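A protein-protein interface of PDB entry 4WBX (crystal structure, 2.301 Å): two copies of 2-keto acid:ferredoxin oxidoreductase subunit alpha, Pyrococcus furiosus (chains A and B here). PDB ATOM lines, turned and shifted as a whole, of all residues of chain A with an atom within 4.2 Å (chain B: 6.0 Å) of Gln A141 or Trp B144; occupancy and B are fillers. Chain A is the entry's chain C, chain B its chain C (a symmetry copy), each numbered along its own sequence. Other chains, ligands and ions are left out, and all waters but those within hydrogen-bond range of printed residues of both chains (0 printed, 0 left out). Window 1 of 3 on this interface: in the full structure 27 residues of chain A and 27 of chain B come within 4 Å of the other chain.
Met A140 touches Trp B144, and with the chains exchanged Trp A144 touches Met B140. Gln A141 touches Trp B144, and with the chains exchanged Trp A144 touches Gln B141. Gln A141 touches Gly B145, and with the chains exchanged Gly A145 touches Gln B141. Trp A144 touches its own counterpart, Trp B144. Positions printed for both chains: 103, 139, 140, 141, 142, 143, 144 and 145. Of the 13 pairs that touch across the chains among the printed residues, 7 have their exchanged pair printed and touching as well.
The side-chain amide oxygen (OE1) of Gln A141 is in hydrogen-bond range of the backbone NH (N) of His B147 (3.2 Å). The side-chain amide oxygen (OE1) of Gln B141 sits close to the backbone carbonyl oxygen (O) of Gly A145 (2.7 Å). The backbone carbonyl oxygen of Gly B145 sits close to the side-chain amide oxygen of Gln A141 (2.7 Å). The side-chain carboxylate (OD2) of Asp A138 sits close to a ring nitrogen (ND1) of His B147. The backbone NH of His B147 sits close to the side-chain hydroxyl of Ser A100 (3.4 Å). The backbone NH of Gly B148 lies within hydrogen-bond range of the side-chain carboxylate of Asp A138 (3.2 Å).
Trp B144 touches Met A140. Gln A141 touches Trp B144 (CA to O, 3.3 Å). Thr B146 touches Gln A141 (C to OE1, 3.4 Å). Trp A144 touches Met B140 (NE1 to CE, 3.3 Å). O of Trp A144 touches CA of Gln B141, at 3.4 Å. CD1 of Trp A144 touches CD1 of Trp B144, at 3.97 Å. CH2 of Trp B144 touches O of Gly A354 (3.9 Å).
Hydrophobic or aromatic side chains of chain B that line the printed part of chain A: Met B140, Trp B144 and His B147. Of the 13 printed residues of chain A, 7 touch a printed residue of chain B.
Phe A99 touches none of the printed residues of chain B. Of the printed residues of chain B, Met A140 touches Trp B144. Gln A141 touches just these residues of chain B: Trp B144 (3.3 Å), Gly B145 (2.7 Å), Thr B146 (3.4 Å) and His B147 (3.2 Å). Printed residues of chain B within 4 Å of Trp A144: Met B140, Gln B141 and Trp B144. Printed residues of chain A within 4 Å of Gly B148: Asp A138. The nearest residue of chain A that does not touch Trp B144 is His A358 (4.03 Å).
OG of Ser A100 lies within hydrogen-bond range of OE1 of Gln A141, at 2.7 Å. A ring nitrogen (ND1) of His B150 lies within hydrogen-bond range of the backbone carbonyl oxygen (O) of Gly B148. The side-chain amide oxygen (OE1) of Gln B103 sits at hydrogen-bond distance from the backbone NH (N) of Thr B146, at 3.4 Å. The backbone carbonyl oxygen (O) of Gly A354 sits close to a ring nitrogen (NE2) of His A358.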
ATOM      1  N   PHE A  99     -25.190 -16.918   5.559  1.00  0.00           N
ATOM      2  CA  PHE A  99     -24.079 -15.979   5.685  1.00  0.00           C
ATOM      3  C   PHE A  99     -24.579 -14.561   5.582  1.00  0.00           C
ATOM      4  O   PHE A  99     -24.061 -13.682   6.260  1.00  0.00           O
ATOM      5  CB  PHE A  99     -23.023 -16.212   4.618  1.00  0.00           C
ATOM      6  CG  PHE A  99     -21.734 -15.479   4.870  1.00  0.00           C
ATOM      7  CD1 PHE A  99     -21.073 -15.613   6.079  1.00  0.00           C
ATOM      8  CD2 PHE A  99     -21.166 -14.698   3.891  1.00  0.00           C
ATOM      9  CE1 PHE A  99     -19.898 -14.987   6.292  1.00  0.00           C
ATOM     10  CE2 PHE A  99     -19.978 -14.052   4.115  1.00  0.00           C
ATOM     11  CZ  PHE A  99     -19.339 -14.192   5.311  1.00  0.00           C
ATOM     12  N   SER A 100     -25.573 -14.351   4.717  1.00  0.00           N
ATOM     13  CA  SER A 100     -26.236 -13.061   4.635  1.00  0.00           C
ATOM     14  C   SER A 100     -26.817 -12.653   5.994  1.00  0.00           C
ATOM     15  O   SER A 100     -26.605 -11.545   6.434  1.00  0.00           O
ATOM     16  CB  SER A 100     -27.333 -13.091   3.573  1.00  0.00           C
ATOM     17  OG  SER A 100     -26.768 -13.235   2.279  1.00  0.00           O
ATOM     18  N   GLN A 103     -24.513 -10.826   8.648  1.00  0.00           N
ATOM     19  CA  GLN A 103     -23.757  -9.599   8.305  1.00  0.00           C
ATOM     20  C   GLN A 103     -23.846  -8.458   9.342  1.00  0.00           C
ATOM     21  O   GLN A 103     -22.852  -7.781   9.577  1.00  0.00           O
ATOM     22  CB  GLN A 103     -24.175  -9.060   6.934  1.00  0.00           C
ATOM     23  CG  GLN A 103     -23.812  -9.975   5.738  1.00  0.00           C
ATOM     24  CD  GLN A 103     -22.340 -10.419   5.700  1.00  0.00           C
ATOM     25  OE1 GLN A 103     -21.432  -9.614   5.465  1.00  0.00           O
ATOM     26  NE2 GLN A 103     -22.107 -11.708   5.928  1.00  0.00           N
ATOM     27  N   ASP A 138     -19.501 -15.909  -3.010  1.00  0.00           N
ATOM     28  CA  ASP A 138     -19.544 -15.077  -1.810  1.00  0.00           C
ATOM     29  C   ASP A 138     -18.224 -14.365  -1.596  1.00  0.00           C
ATOM     30  O   ASP A 138     -17.913 -13.993  -0.459  1.00  0.00           O
ATOM     31  CB  ASP A 138     -19.855 -15.883  -0.533  1.00  0.00           C
ATOM     32  CG  ASP A 138     -21.220 -16.567  -0.561  1.00  0.00           C
ATOM     33  OD1 ASP A 138     -22.049 -16.273  -1.456  1.00  0.00           O
ATOM     34  OD2 ASP A 138     -21.477 -17.390   0.346  1.00  0.00           O
ATOM     35  N   ILE A 139     -17.439 -14.167  -2.650  1.00  0.00           N
ATOM     36  CA  ILE A 139     -16.172 -13.457  -2.469  1.00  0.00           C
ATOM     37  C   ILE A 139     -16.392 -11.981  -2.124  1.00  0.00           C
ATOM     38  O   ILE A 139     -15.795 -11.456  -1.176  1.00  0.00           O
ATOM     39  CB  ILE A 139     -15.266 -13.528  -3.709  1.00  0.00           C
ATOM     40  CG1 ILE A 139     -15.020 -14.988  -4.103  1.00  0.00           C
ATOM     41  CG2 ILE A 139     -13.949 -12.777  -3.435  1.00  0.00           C
ATOM     42  CD1 ILE A 139     -14.576 -15.152  -5.537  1.00  0.00           C
ATOM     43  N   MET A 140     -17.250 -11.311  -2.887  1.00  0.00           N
ATOM     44  CA  MET A 140     -17.524  -9.907  -2.612  1.00  0.00           C
ATOM     45  C   MET A 140     -18.305  -9.730  -1.301  1.00  0.00           C
ATOM     46  O   MET A 140     -17.996  -8.840  -0.492  1.00  0.00           O
ATOM     47  CB  MET A 140     -18.282  -9.266  -3.782  1.00  0.00           C
ATOM     48  CG  MET A 140     -17.435  -9.131  -5.069  1.00  0.00           C
ATOM     49  SD  MET A 140     -15.843  -8.310  -4.782  1.00  0.00           S
ATOM     50  CE  MET A 140     -16.173  -6.700  -5.467  1.00  0.00           C
ATOM     51  N   GLN A 141     -19.299 -10.579  -1.077  1.00  0.00           N
ATOM     52  CA  GLN A 141     -20.093 -10.446   0.130  1.00  0.00           C
ATOM     53  C   GLN A 141     -19.216 -10.648   1.348  1.00  0.00           C
ATOM     54  O   GLN A 141     -19.437 -10.034   2.384  1.00  0.00           O
ATOM     55  CB  GLN A 141     -21.258 -11.429   0.139  1.00  0.00           C
ATOM     56  CG  GLN A 141     -22.117 -11.349   1.386  1.00  0.00           C
ATOM     57  CD  GLN A 141     -23.199 -12.420   1.429  1.00  0.00           C
ATOM     58  OE1 GLN A 141     -24.373 -12.133   1.704  1.00  0.00           O
ATOM     59  NE2 GLN A 141     -22.802 -13.665   1.177  1.00  0.00           N
ATOM     60  N   ALA A 142     -18.193 -11.477   1.228  1.00  0.00           N
ATOM     61  CA  ALA A 142     -17.285 -11.646   2.356  1.00  0.00           C
ATOM     62  C   ALA A 142     -16.584 -10.324   2.681  1.00  0.00           C
ATOM     63  O   ALA A 142     -16.334 -10.020   3.846  1.00  0.00           O
ATOM     64  CB  ALA A 142     -16.258 -12.755   2.071  1.00  0.00           C
ATOM     65  N   ILE A 143     -16.275  -9.538   1.650  1.00  0.00           N
ATOM     66  CA  ILE A 143     -15.532  -8.281   1.814  1.00  0.00           C
ATOM     67  C   ILE A 143     -16.419  -7.109   2.241  1.00  0.00           C
ATOM     68  O   ILE A 143     -16.086  -6.351   3.159  1.00  0.00           O
ATOM     69  CB  ILE A 143     -14.818  -7.883   0.502  1.00  0.00           C
ATOM     70  CG1 ILE A 143     -13.560  -8.706   0.287  1.00  0.00           C
ATOM     71  CG2 ILE A 143     -14.409  -6.421   0.512  1.00  0.00           C
ATOM     72  CD1 ILE A 143     -13.164  -8.751  -1.169  1.00  0.00           C
ATOM     73  N   TRP A 144     -17.552  -6.970   1.559  1.00  0.00           N
ATOM     74  CA  TRP A 144     -18.349  -5.750   1.617  1.00  0.00           C
ATOM     75  C   TRP A 144     -19.775  -5.909   2.174  1.00  0.00           C
ATOM     76  O   TRP A 144     -20.595  -5.002   2.031  1.00  0.00           O
ATOM     77  CB  TRP A 144     -18.486  -5.164   0.218  1.00  0.00           C
ATOM     78  CG  TRP A 144     -17.248  -4.742  -0.505  1.00  0.00           C
ATOM     79  CD1 TRP A 144     -16.725  -5.316  -1.631  1.00  0.00           C
ATOM     80  CD2 TRP A 144     -16.435  -3.595  -0.222  1.00  0.00           C
ATOM     81  NE1 TRP A 144     -15.617  -4.621  -2.038  1.00  0.00           N
ATOM     82  CE2 TRP A 144     -15.418  -3.556  -1.196  1.00  0.00           C
ATOM     83  CE3 TRP A 144     -16.462  -2.600   0.770  1.00  0.00           C
ATOM     84  CZ2 TRP A 144     -14.428  -2.562  -1.209  1.00  0.00           C
ATOM     85  CZ3 TRP A 144     -15.477  -1.616   0.758  1.00  0.00           C
ATOM     86  CH2 TRP A 144     -14.478  -1.605  -0.227  1.00  0.00           C
ATOM     87  N   GLY A 145     -20.090  -7.051   2.769  1.00  0.00           N
ATOM     88  CA  GLY A 145     -21.453  -7.317   3.198  1.00  0.00           C
ATOM     89  C   GLY A 145     -21.854  -6.610   4.479  1.00  0.00           C
ATOM     90  O   GLY A 145     -23.030  -6.390   4.725  1.00  0.00           O
ATOM     91  N   GLY A 354     -17.890 -13.126 -11.866  1.00  0.00           N
ATOM     92  CA  GLY A 354     -16.863 -12.106 -11.817  1.00  0.00           C
ATOM     93  C   GLY A 354     -16.867 -11.397 -10.483  1.00  0.00           C
ATOM     94  O   GLY A 354     -17.761 -10.597 -10.202  1.00  0.00           O
ATOM     95  N   HIS A 358     -12.807  -8.592 -10.616  1.00  0.00           N
ATOM     96  CA  HIS A 358     -12.858  -7.144 -10.434  1.00  0.00           C
ATOM     97  C   HIS A 358     -11.658  -6.644  -9.663  1.00  0.00           C
ATOM     98  O   HIS A 358     -11.098  -5.618 -10.005  1.00  0.00           O
ATOM     99  CB  HIS A 358     -14.137  -6.717  -9.709  1.00  0.00           C
ATOM    100  CG  HIS A 358     -15.387  -6.904 -10.509  1.00  0.00           C
ATOM    101  ND1 HIS A 358     -15.949  -5.892 -11.257  1.00  0.00           N
ATOM    102  CD2 HIS A 358     -16.199  -7.978 -10.661  1.00  0.00           C
ATOM    103  CE1 HIS A 358     -17.043  -6.341 -11.847  1.00  0.00           C
ATOM    104  NE2 HIS A 358     -17.219  -7.605 -11.502  1.00  0.00           N
ATOM    105  N   GLN B 103     -30.458  -8.348   3.812  1.00  0.00           N
ATOM    106  CA  GLN B 103     -29.696  -8.867   2.652  1.00  0.00           C
ATOM    107  C   GLN B 103     -30.137 -10.255   2.141  1.00  0.00           C
ATOM    108  O   GLN B 103     -30.151 -10.475   0.935  1.00  0.00           O
ATOM    109  CB  GLN B 103     -28.194  -8.899   2.950  1.00  0.00           C
ATOM    110  CG  GLN B 103     -27.538  -7.509   3.137  1.00  0.00           C
ATOM    111  CD  GLN B 103     -27.824  -6.512   2.002  1.00  0.00           C
ATOM    112  OE1 GLN B 103     -27.353  -6.674   0.871  1.00  0.00           O
ATOM    113  NE2 GLN B 103     -28.598  -5.475   2.309  1.00  0.00           N
ATOM    114  N   ILE B 139     -22.335   2.085   0.064  1.00  0.00           N
ATOM    115  CA  ILE B 139     -22.311   1.977  -1.395  1.00  0.00           C
ATOM    116  C   ILE B 139     -21.975   0.555  -1.855  1.00  0.00           C
ATOM    117  O   ILE B 139     -22.660  -0.011  -2.716  1.00  0.00           O
ATOM    118  CB  ILE B 139     -21.306   2.940  -2.047  1.00  0.00           C
ATOM    119  CG1 ILE B 139     -21.593   4.381  -1.612  1.00  0.00           C
ATOM    120  CG2 ILE B 139     -21.352   2.782  -3.579  1.00  0.00           C
ATOM    121  CD1 ILE B 139     -20.410   5.304  -1.788  1.00  0.00           C
ATOM    122  N   MET B 140     -20.926  -0.026  -1.281  1.00  0.00           N
ATOM    123  CA  MET B 140     -20.553  -1.383  -1.654  1.00  0.00           C
ATOM    124  C   MET B 140     -21.588  -2.408  -1.167  1.00  0.00           C
ATOM    125  O   MET B 140     -21.967  -3.331  -1.907  1.00  0.00           O
ATOM    126  CB  MET B 140     -19.158  -1.728  -1.115  1.00  0.00           C
ATOM    127  CG  MET B 140     -18.018  -0.936  -1.795  1.00  0.00           C
ATOM    128  SD  MET B 140     -18.071  -1.038  -3.606  1.00  0.00           S
ATOM    129  CE  MET B 140     -16.741  -2.181  -3.911  1.00  0.00           C
ATOM    130  N   GLN B 141     -22.061  -2.244   0.062  1.00  0.00           N
ATOM    131  CA  GLN B 141     -23.021  -3.195   0.591  1.00  0.00           C
ATOM    132  C   GLN B 141     -24.283  -3.173  -0.246  1.00  0.00           C
ATOM    133  O   GLN B 141     -24.935  -4.195  -0.417  1.00  0.00           O
ATOM    134  CB  GLN B 141     -23.342  -2.905   2.053  1.00  0.00           C
ATOM    135  CG  GLN B 141     -24.353  -3.859   2.658  1.00  0.00           C
ATOM    136  CD  GLN B 141     -24.749  -3.477   4.078  1.00  0.00           C
ATOM    137  OE1 GLN B 141     -24.769  -4.321   4.985  1.00  0.00           O
ATOM    138  NE2 GLN B 141     -25.086  -2.204   4.271  1.00  0.00           N
ATOM    139  N   ALA B 142     -24.619  -2.023  -0.806  1.00  0.00           N
ATOM    140  CA  ALA B 142     -25.788  -1.977  -1.675  1.00  0.00           C
ATOM    141  C   ALA B 142     -25.583  -2.875  -2.897  1.00  0.00           C
ATOM    142  O   ALA B 142     -26.526  -3.503  -3.376  1.00  0.00           O
ATOM    143  CB  ALA B 142     -26.095  -0.531  -2.103  1.00  0.00           C
ATOM    144  N   ILE B 143     -24.348  -2.941  -3.394  1.00  0.00           N
ATOM    145  CA  ILE B 143     -24.029  -3.703  -4.611  1.00  0.00           C
ATOM    146  C   ILE B 143     -23.837  -5.198  -4.350  1.00  0.00           C
ATOM    147  O   ILE B 143     -24.371  -6.051  -5.068  1.00  0.00           O
ATOM    148  CB  ILE B 143     -22.742  -3.167  -5.279  1.00  0.00           C
ATOM    149  CG1 ILE B 143     -23.011  -1.882  -6.043  1.00  0.00           C
ATOM    150  CG2 ILE B 143     -22.167  -4.170  -6.263  1.00  0.00           C
ATOM    151  CD1 ILE B 143     -21.755  -1.066  -6.224  1.00  0.00           C
ATOM    152  N   TRP B 144     -23.060  -5.504  -3.314  1.00  0.00           N
ATOM    153  CA  TRP B 144     -22.523  -6.845  -3.116  1.00  0.00           C
ATOM    154  C   TRP B 144     -22.964  -7.557  -1.824  1.00  0.00           C
ATOM    155  O   TRP B 144     -22.376  -8.573  -1.451  1.00  0.00           O
ATOM    156  CB  TRP B 144     -21.002  -6.785  -3.087  1.00  0.00           C
ATOM    157  CG  TRP B 144     -20.283  -6.294  -4.302  1.00  0.00           C
ATOM    158  CD1 TRP B 144     -19.559  -5.138  -4.410  1.00  0.00           C
ATOM    159  CD2 TRP B 144     -20.124  -6.987  -5.546  1.00  0.00           C
ATOM    160  NE1 TRP B 144     -18.997  -5.053  -5.656  1.00  0.00           N
ATOM    161  CE2 TRP B 144     -19.322  -6.177  -6.374  1.00  0.00           C
ATOM    162  CE3 TRP B 144     -20.592  -8.214  -6.048  1.00  0.00           C
ATOM    163  CZ2 TRP B 144     -18.977  -6.548  -7.682  1.00  0.00           C
ATOM    164  CZ3 TRP B 144     -20.253  -8.579  -7.348  1.00  0.00           C
ATOM    165  CH2 TRP B 144     -19.451  -7.750  -8.146  1.00  0.00           C
ATOM    166  N   GLY B 145     -23.957  -7.025  -1.124  1.00  0.00           N
ATOM    167  CA  GLY B 145     -24.333  -7.571   0.169  1.00  0.00           C
ATOM    168  C   GLY B 145     -25.152  -8.847   0.095  1.00  0.00           C
ATOM    169  O   GLY B 145     -25.174  -9.626   1.035  1.00  0.00           O
ATOM    170  N   THR B 146     -25.852  -9.025  -1.017  1.00  0.00           N
ATOM    171  CA  THR B 146     -26.495 -10.272  -1.367  1.00  0.00           C
ATOM    172  C   THR B 146     -25.504 -11.446  -1.431  1.00  0.00           C
ATOM    173  O   THR B 146     -24.362 -11.283  -1.846  1.00  0.00           O
ATOM    174  CB  THR B 146     -27.193 -10.110  -2.718  1.00  0.00           C
ATOM    175  OG1 THR B 146     -28.396  -9.376  -2.515  1.00  0.00           O
ATOM    176  CG2 THR B 146     -27.565 -11.409  -3.321  1.00  0.00           C
ATOM    177  N   HIS B 147     -25.931 -12.630  -1.004  1.00  0.00           N
ATOM    178  CA  HIS B 147     -25.137 -13.826  -1.238  1.00  0.00           C
ATOM    179  C   HIS B 147     -25.309 -14.277  -2.694  1.00  0.00           C
ATOM    180  O   HIS B 147     -26.412 -14.196  -3.257  1.00  0.00           O
ATOM    181  CB  HIS B 147     -25.535 -14.953  -0.275  1.00  0.00           C
ATOM    182  CG  HIS B 147     -25.477 -16.320  -0.895  1.00  0.00           C
ATOM    183  ND1 HIS B 147     -24.290 -16.963  -1.171  1.00  0.00           N
ATOM    184  CD2 HIS B 147     -26.467 -17.147  -1.317  1.00  0.00           C
ATOM    185  CE1 HIS B 147     -24.548 -18.138  -1.732  1.00  0.00           C
ATOM    186  NE2 HIS B 147     -25.858 -18.272  -1.829  1.00  0.00           N
ATOM    187  N   GLY B 148     -24.217 -14.730  -3.300  1.00  0.00           N
ATOM    188  CA  GLY B 148     -24.269 -15.335  -4.617  1.00  0.00           C
ATOM    189  C   GLY B 148     -24.001 -14.397  -5.784  1.00  0.00           C
ATOM    190  O   GLY B 148     -23.447 -13.310  -5.622  1.00  0.00           O
ATOM    191  N   HIS B 150     -25.729 -12.197  -8.683  1.00  0.00           N
ATOM    192  CA  HIS B 150     -26.992 -11.491  -8.733  1.00  0.00           C
ATOM    193  C   HIS B 150     -26.734 -10.194  -9.460  1.00  0.00           C
ATOM    194  O   HIS B 150     -25.584  -9.820  -9.679  1.00  0.00           O
ATOM    195  CB  HIS B 150     -27.498 -11.200  -7.325  1.00  0.00           C
ATOM    196  CG  HIS B 150     -26.558 -10.324  -6.565  1.00  0.00           C
ATOM    197  ND1 HIS B 150     -25.512 -10.829  -5.824  1.00  0.00           N
ATOM    198  CD2 HIS B 150     -26.435  -8.978  -6.521  1.00  0.00           C
ATOM    199  CE1 HIS B 150     -24.816  -9.830  -5.309  1.00  0.00           C
ATOM    200  NE2 HIS B 150     -25.353  -8.698  -5.719  1.00  0.00           N
ATOM    201  N   TRP B 329     -25.430   1.170  -9.657  1.00  0.00           N
ATOM    202  CA  TRP B 329     -25.315  -0.170 -10.224  1.00  0.00           C
ATOM    203  C   TRP B 329     -26.568  -0.488 -11.027  1.00  0.00           C
ATOM    204  O   TRP B 329     -27.665  -0.135 -10.617  1.00  0.00           O
ATOM    205  CB  TRP B 329     -25.106  -1.200  -9.113  1.00  0.00           C
ATOM    206  CG  TRP B 329     -24.581  -2.488  -9.609  1.00  0.00           C
ATOM    207  CD1 TRP B 329     -25.307  -3.575 -10.014  1.00  0.00           C
ATOM    208  CD2 TRP B 329     -23.197  -2.844  -9.761  1.00  0.00           C
ATOM    209  NE1 TRP B 329     -24.452  -4.583 -10.419  1.00  0.00           N
ATOM    210  CE2 TRP B 329     -23.158  -4.160 -10.267  1.00  0.00           C
ATOM    211  CE3 TRP B 329     -21.989  -2.176  -9.518  1.00  0.00           C
ATOM    212  CZ2 TRP B 329     -21.959  -4.814 -10.546  1.00  0.00           C
ATOM    213  CZ3 TRP B 329     -20.796  -2.834  -9.793  1.00  0.00           C
ATOM    214  CH2 TRP B 329     -20.793  -4.140 -10.304  1.00  0.00           C
